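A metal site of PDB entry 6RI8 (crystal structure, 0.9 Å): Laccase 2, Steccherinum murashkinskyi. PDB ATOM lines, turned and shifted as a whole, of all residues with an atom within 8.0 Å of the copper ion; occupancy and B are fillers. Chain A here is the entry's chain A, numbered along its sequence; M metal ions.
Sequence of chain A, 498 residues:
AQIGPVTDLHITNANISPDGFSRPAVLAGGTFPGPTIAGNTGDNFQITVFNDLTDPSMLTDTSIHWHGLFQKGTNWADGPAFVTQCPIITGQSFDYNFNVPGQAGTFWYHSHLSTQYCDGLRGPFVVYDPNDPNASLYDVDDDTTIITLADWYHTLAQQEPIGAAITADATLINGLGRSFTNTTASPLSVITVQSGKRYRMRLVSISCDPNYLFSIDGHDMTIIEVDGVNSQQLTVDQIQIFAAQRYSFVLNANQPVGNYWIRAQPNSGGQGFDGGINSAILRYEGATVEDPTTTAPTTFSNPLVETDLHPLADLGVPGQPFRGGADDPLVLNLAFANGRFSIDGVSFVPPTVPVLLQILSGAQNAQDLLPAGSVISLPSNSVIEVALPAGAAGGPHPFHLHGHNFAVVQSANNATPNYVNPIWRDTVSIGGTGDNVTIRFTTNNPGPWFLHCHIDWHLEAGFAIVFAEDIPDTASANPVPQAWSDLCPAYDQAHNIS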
ATOM      1  N   CYS A 208       5.040   6.864   1.413  1.00  0.00           N
ATOM      2  CA  CYS A 208       4.036   5.812   1.519  1.00  0.00           C
ATOM      3  C   CYS A 208       4.359   4.778   2.569  1.00  0.00           C
ATOM      4  O   CYS A 208       3.475   3.957   2.880  1.00  0.00           O
ATOM      5  CB  CYS A 208       3.813   5.104   0.186  1.00  0.00           C
ATOM      6  SG  CYS A 208       2.452   5.892  -0.743  1.00  0.00           S
ATOM      7  N   ASP A 209       5.584   4.734   3.091  1.00  0.00           N
ATOM      8  CA  ASP A 209       5.963   3.643   4.004  1.00  0.00           C
ATOM      9  C   ASP A 209       7.162   3.997   4.859  1.00  0.00           C
ATOM     10  O   ASP A 209       6.984   4.209   6.057  1.00  0.00           O
ATOM     11  CB  ASP A 209       6.092   2.328   3.232  1.00  0.00           C
ATOM     12  CG  ASP A 209       6.632   1.192   4.025  1.00  0.00           C
ATOM     13  OD1 ASP A 209       7.005   1.305   5.174  1.00  0.00           O
ATOM     14  OD2 ASP A 209       6.782   0.093   3.401  1.00  0.00           O
ATOM     15  N   PHE A 341      -4.801  -5.977   8.467  1.00  0.00           N
ATOM     16  CA  PHE A 341      -4.799  -5.284   9.736  1.00  0.00           C
ATOM     17  C   PHE A 341      -6.198  -5.158  10.282  1.00  0.00           C
ATOM     18  O   PHE A 341      -7.194  -5.161   9.537  1.00  0.00           O
ATOM     19  CB  PHE A 341      -4.207  -3.887   9.563  1.00  0.00           C
ATOM     20  CG  PHE A 341      -2.733  -3.892   9.335  1.00  0.00           C
ATOM     21  CD1 PHE A 341      -2.201  -3.921   8.047  1.00  0.00           C
ATOM     22  CD2 PHE A 341      -1.847  -3.886  10.396  1.00  0.00           C
ATOM     23  CE1 PHE A 341      -0.838  -3.950   7.852  1.00  0.00           C
ATOM     24  CE2 PHE A 341      -0.485  -3.900  10.201  1.00  0.00           C
ATOM     25  CZ  PHE A 341       0.049  -3.945   8.933  1.00  0.00           C
ATOM     26  N   ALA A 392       1.717  -4.954  16.478  1.00  0.00           N
ATOM     27  CA  ALA A 392       1.305  -5.453  15.160  1.00  0.00           C
ATOM     28  C   ALA A 392       2.483  -5.429  14.193  1.00  0.00           C
ATOM     29  O   ALA A 392       3.231  -4.432  14.162  1.00  0.00           O
ATOM     30  CB  ALA A 392       0.168  -4.626  14.606  1.00  0.00           C
ATOM     31  N   ALA A 393       2.609  -6.471  13.373  1.00  0.00           N
ATOM     32  CA  ALA A 393       3.679  -6.565  12.380  1.00  0.00           C
ATOM     33  C   ALA A 393       3.705  -5.353  11.471  1.00  0.00           C
ATOM     34  O   ALA A 393       2.707  -4.666  11.243  1.00  0.00           O
ATOM     35  CB  ALA A 393       3.478  -7.838  11.555  1.00  0.00           C
ATOM     36  N   GLY A 394       4.899  -5.120  10.922  1.00  0.00           N
ATOM     37  CA  GLY A 394       5.094  -4.058   9.954  1.00  0.00           C
ATOM     38  C   GLY A 394       5.418  -2.710  10.560  1.00  0.00           C
ATOM     39  O   GLY A 394       5.470  -1.731   9.832  1.00  0.00           O
ATOM     40  N   GLY A 395       5.635  -2.640  11.862  1.00  0.00           N
ATOM     41  CA  GLY A 395       5.880  -1.373  12.525  1.00  0.00           C
ATOM     42  C   GLY A 395       7.297  -0.885  12.308  1.00  0.00           C
ATOM     43  O   GLY A 395       8.140  -1.584  11.699  1.00  0.00           O
ATOM     44  N   PRO A 396       7.619   0.308  12.802  1.00  0.00           N
ATOM     45  CA  PRO A 396       6.755   1.150  13.654  1.00  0.00           C
ATOM     46  C   PRO A 396       5.706   1.869  12.818  1.00  0.00           C
ATOM     47  O   PRO A 396       5.990   2.468  11.770  1.00  0.00           O
ATOM     48  CB  PRO A 396       7.740   2.119  14.295  1.00  0.00           C
ATOM     49  CG  PRO A 396       8.879   2.193  13.303  1.00  0.00           C
ATOM     50  CD  PRO A 396       8.988   0.846  12.721  1.00  0.00           C
ATOM     51  N   HIS A 397       4.470   1.839  13.305  1.00  0.00           N
ATOM     52  CA  HIS A 397       3.329   2.395  12.579  1.00  0.00           C
ATOM     53  C   HIS A 397       3.099   3.846  12.924  1.00  0.00           C
ATOM     54  O   HIS A 397       2.858   4.156  14.102  1.00  0.00           O
ATOM     55  CB  HIS A 397       2.053   1.602  12.887  1.00  0.00           C
ATOM     56  CG  HIS A 397       2.164   0.147  12.587  1.00  0.00           C
ATOM     57  ND1 HIS A 397       2.078  -0.336  11.308  1.00  0.00           N
ATOM     58  CD2 HIS A 397       2.347  -0.913  13.430  1.00  0.00           C
ATOM     59  CE1 HIS A 397       2.243  -1.640  11.379  1.00  0.00           C
ATOM     60  NE2 HIS A 397       2.386  -2.026  12.638  1.00  0.00           N
ATOM     61  N   PRO A 398       3.089   4.758  11.922  1.00  0.00           N
ATOM     62  CA  PRO A 398       2.788   6.169  12.186  1.00  0.00           C
ATOM     63  C   PRO A 398       1.302   6.429  12.073  1.00  0.00           C
ATOM     64  O   PRO A 398       0.754   6.566  10.970  1.00  0.00           O
ATOM     65  CB  PRO A 398       3.603   6.885  11.107  1.00  0.00           C
ATOM     66  CG  PRO A 398       3.592   5.914   9.936  1.00  0.00           C
ATOM     67  CD  PRO A 398       3.574   4.533  10.561  1.00  0.00           C
ATOM     68  N   PHE A 399       0.612   6.512  13.200  1.00  0.00           N
ATOM     69  CA  PHE A 399      -0.812   6.751  13.213  1.00  0.00           C
ATOM     70  C   PHE A 399      -1.136   8.214  13.080  1.00  0.00           C
ATOM     71  O   PHE A 399      -0.494   9.090  13.677  1.00  0.00           O
ATOM     72  CB  PHE A 399      -1.471   6.170  14.488  1.00  0.00           C
ATOM     73  CG  PHE A 399      -1.985   4.773  14.267  1.00  0.00           C
ATOM     74  CD1 PHE A 399      -1.120   3.700  14.089  1.00  0.00           C
ATOM     75  CD2 PHE A 399      -3.358   4.545  14.121  1.00  0.00           C
ATOM     76  CE1 PHE A 399      -1.616   2.439  13.777  1.00  0.00           C
ATOM     77  CE2 PHE A 399      -3.833   3.279  13.798  1.00  0.00           C
ATOM     78  CZ  PHE A 399      -2.963   2.240  13.633  1.00  0.00           C
ATOM     79  N   ILE A 430       3.804   4.814  16.808  1.00  0.00           N
ATOM     80  CA  ILE A 430       3.363   4.082  17.992  1.00  0.00           C
ATOM     81  C   ILE A 430       4.449   3.168  18.540  1.00  0.00           C
ATOM     82  O   ILE A 430       4.267   2.506  19.559  1.00  0.00           O
ATOM     83  CB  ILE A 430       2.029   3.378  17.777  1.00  0.00           C
ATOM     84  CG1 ILE A 430       2.146   2.175  16.834  1.00  0.00           C
ATOM     85  CG2 ILE A 430       0.970   4.372  17.324  1.00  0.00           C
ATOM     86  CD1 ILE A 430       0.897   1.334  16.795  1.00  0.00           C
ATOM     87  N   HIS A 452      -5.826   6.334  11.115  1.00  0.00           N
ATOM     88  CA  HIS A 452      -5.244   5.199  10.441  1.00  0.00           C
ATOM     89  C   HIS A 452      -3.736   5.259  10.488  1.00  0.00           C
ATOM     90  O   HIS A 452      -3.126   6.316  10.668  1.00  0.00           O
ATOM     91  CB  HIS A 452      -5.708   5.143   8.969  1.00  0.00           C
ATOM     92  CG  HIS A 452      -5.338   6.326   8.134  1.00  0.00           C
ATOM     93  ND1 HIS A 452      -4.141   6.426   7.464  1.00  0.00           N
ATOM     94  CD2 HIS A 452      -6.031   7.441   7.837  1.00  0.00           C
ATOM     95  CE1 HIS A 452      -4.139   7.581   6.812  1.00  0.00           C
ATOM     96  NE2 HIS A 452      -5.277   8.241   6.998  1.00  0.00           N
ATOM     97  N   CYS A 453      -3.116   4.098  10.252  1.00  0.00           N
ATOM     98  CA  CYS A 453      -1.692   4.072   9.974  1.00  0.00           C
ATOM     99  C   CYS A 453      -1.430   4.756   8.643  1.00  0.00           C
ATOM    100  O   CYS A 453      -2.142   4.496   7.676  1.00  0.00           O
ATOM    101  CB  CYS A 453      -1.198   2.626   9.921  1.00  0.00           C
ATOM    102  SG  CYS A 453       0.607   2.623   9.631  1.00  0.00           S
ATOM    103  N   HIS A 454      -0.412   5.620   8.591  1.00  0.00           N
ATOM    104  CA  HIS A 454      -0.092   6.341   7.371  1.00  0.00           C
ATOM    105  C   HIS A 454       0.912   5.631   6.483  1.00  0.00           C
ATOM    106  O   HIS A 454       1.320   6.170   5.466  1.00  0.00           O
ATOM    107  CB  HIS A 454       0.343   7.790   7.680  1.00  0.00           C
ATOM    108  CG  HIS A 454      -0.118   8.772   6.651  1.00  0.00           C
ATOM    109  ND1 HIS A 454       0.271   8.751   5.339  1.00  0.00           N
ATOM    110  CD2 HIS A 454      -0.944   9.854   6.748  1.00  0.00           C
ATOM    111  CE1 HIS A 454      -0.320   9.750   4.698  1.00  0.00           C
ATOM    112  NE2 HIS A 454      -1.057  10.467   5.516  1.00  0.00           N
ATOM    113  N   ILE A 455       1.281   4.374   6.822  1.00  0.00           N
ATOM    114  CA  ILE A 455       1.922   3.510   5.825  1.00  0.00           C
ATOM    115  C   ILE A 455       0.781   3.095   4.903  1.00  0.00           C
ATOM    116  O   ILE A 455      -0.149   2.392   5.305  1.00  0.00           O
ATOM    117  CB  ILE A 455       2.644   2.338   6.498  1.00  0.00           C
ATOM    118  CG1 ILE A 455       3.805   2.847   7.337  1.00  0.00           C
ATOM    119  CG2 ILE A 455       3.079   1.326   5.438  1.00  0.00           C
ATOM    120  CD1 ILE A 455       4.414   1.831   8.277  1.00  0.00           C
ATOM    121  N   ASP A 456       0.830   3.590   3.655  1.00  0.00           N
ATOM    122  CA  ASP A 456      -0.355   3.492   2.810  1.00  0.00           C
ATOM    123  C   ASP A 456      -0.720   2.047   2.509  1.00  0.00           C
ATOM    124  O   ASP A 456      -1.896   1.710   2.347  1.00  0.00           O
ATOM    125  CB  ASP A 456      -0.150   4.330   1.553  1.00  0.00           C
ATOM    126  CG  ASP A 456      -1.431   4.937   0.988  1.00  0.00           C
ATOM    127  OD1 ASP A 456      -2.283   5.326   1.814  1.00  0.00           O
ATOM    128  OD2 ASP A 456      -1.523   5.087  -0.222  1.00  0.00           O
ATOM    129  N   TRP A 457       0.293   1.171   2.441  1.00  0.00           N
ATOM    130  CA  TRP A 457       0.056  -0.230   2.209  1.00  0.00           C
ATOM    131  C   TRP A 457      -0.761  -0.853   3.366  1.00  0.00           C
ATOM    132  O   TRP A 457      -1.506  -1.803   3.169  1.00  0.00           O
ATOM    133  CB  TRP A 457       1.383  -0.965   2.019  1.00  0.00           C
ATOM    134  CG  TRP A 457       2.317  -0.295   1.063  1.00  0.00           C
ATOM    135  CD1 TRP A 457       3.511   0.303   1.355  1.00  0.00           C
ATOM    136  CD2 TRP A 457       2.124  -0.099  -0.340  1.00  0.00           C
ATOM    137  NE1 TRP A 457       4.057   0.870   0.264  1.00  0.00           N
ATOM    138  CE2 TRP A 457       3.240   0.656  -0.815  1.00  0.00           C
ATOM    139  CE3 TRP A 457       1.144  -0.471  -1.255  1.00  0.00           C
ATOM    140  CZ2 TRP A 457       3.371   1.027  -2.146  1.00  0.00           C
ATOM    141  CZ3 TRP A 457       1.284  -0.109  -2.557  1.00  0.00           C
ATOM    142  CH2 TRP A 457       2.373   0.641  -2.982  1.00  0.00           C
ATOM    143  N   HIS A 458      -0.546  -0.321   4.574  1.00  0.00           N
ATOM    144  CA  HIS A 458      -1.263  -0.820   5.757  1.00  0.00           C
ATOM    145  C   HIS A 458      -2.696  -0.279   5.814  1.00  0.00           C
ATOM    146  O   HIS A 458      -3.605  -1.014   6.183  1.00  0.00           O
ATOM    147  CB  HIS A 458      -0.484  -0.446   7.031  1.00  0.00           C
ATOM    148  CG  HIS A 458       0.872  -1.043   7.102  1.00  0.00           C
ATOM    149  ND1 HIS A 458       1.705  -0.735   8.169  1.00  0.00           N
ATOM    150  CD2 HIS A 458       1.498  -1.915   6.286  1.00  0.00           C
ATOM    151  CE1 HIS A 458       2.823  -1.428   7.940  1.00  0.00           C
ATOM    152  NE2 HIS A 458       2.729  -2.154   6.833  1.00  0.00           N
ATOM    153  N   LEU A 459      -2.883   1.003   5.471  1.00  0.00           N
ATOM    154  CA  LEU A 459      -4.216   1.531   5.313  1.00  0.00           C
ATOM    155  C   LEU A 459      -5.014   0.677   4.333  1.00  0.00           C
ATOM    156  O   LEU A 459      -6.173   0.292   4.598  1.00  0.00           O
ATOM    157  CB  LEU A 459      -4.153   2.983   4.883  1.00  0.00           C
ATOM    158  CG  LEU A 459      -5.480   3.610   4.472  1.00  0.00           C
ATOM    159  CD1 LEU A 459      -6.518   3.563   5.552  1.00  0.00           C
ATOM    160  CD2 LEU A 459      -5.260   5.031   4.003  1.00  0.00           C
ATOM    161  N   PHE A 463      -5.922  -0.975   8.132  1.00  0.00           N
ATOM    162  CA  PHE A 463      -5.467  -0.475   9.459  1.00  0.00           C
ATOM    163  C   PHE A 463      -6.058   0.926   9.733  1.00  0.00           C
ATOM    164  O   PHE A 463      -5.330   1.926   9.734  1.00  0.00           O
ATOM    165  CB  PHE A 463      -3.962  -0.495   9.520  1.00  0.00           C
ATOM    166  CG  PHE A 463      -3.347  -0.743  10.902  1.00  0.00           C
ATOM    167  CD1 PHE A 463      -4.075  -1.241  11.985  1.00  0.00           C
ATOM    168  CD2 PHE A 463      -1.976  -0.593  11.052  1.00  0.00           C
ATOM    169  CE1 PHE A 463      -3.441  -1.579  13.169  1.00  0.00           C
ATOM    170  CE2 PHE A 463      -1.335  -0.923  12.236  1.00  0.00           C
ATOM    171  CZ  PHE A 463      -2.064  -1.432  13.278  1.00  0.00           C
HETATM  172 CU    CU M   1       1.373   0.570   9.630  1.00  0.00          CU
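SG of Cys 453 sits close to N of Ile 455, 3.4 Å away.
The backbone carbonyl oxygen (O) of His 458 lies within hydrogen-bond range of the backbone NH (N) of Phe 463 (3.0 Å).
A ring nitrogen (NE2) of His 397 is in hydrogen-bond range of the backbone carbonyl oxygen (O) of Ala 393 (3.0 Å).
The backbone carbonyl oxygen (O) of Ala 392 lies within hydrogen-bond range of a ring nitrogen (NE2) of His 397.
The backbone carbonyl oxygen of Phe 463 is in hydrogen-bond range of the backbone NH of Cys 453, 3.1 Å away.
O of His 397 is in hydrogen-bond range of N of Ile 430 (2.9 Å).
A ring nitrogen (NE2) of His 397 lies within hydrogen-bond range of the backbone NH (N) of Gly 395, 3.4 Å away.
Residues that only touch the copper ion: Ile 455 and Phe 463.
Of the 21 residues printed, 5 come within 4 Å of the copper ion.
The nearest printed residue that does not touch the copper ion is Pro 398 (4.6 Å).
ND1 of His 458 binds the copper ion (2.0 Å).
ND1 of His 397 binds the copper ion.
The side-chain sulfur (SG) of Cys 453 binds the copper ion (2.2 Å).
The copper ion has three donor atoms within binding distance.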
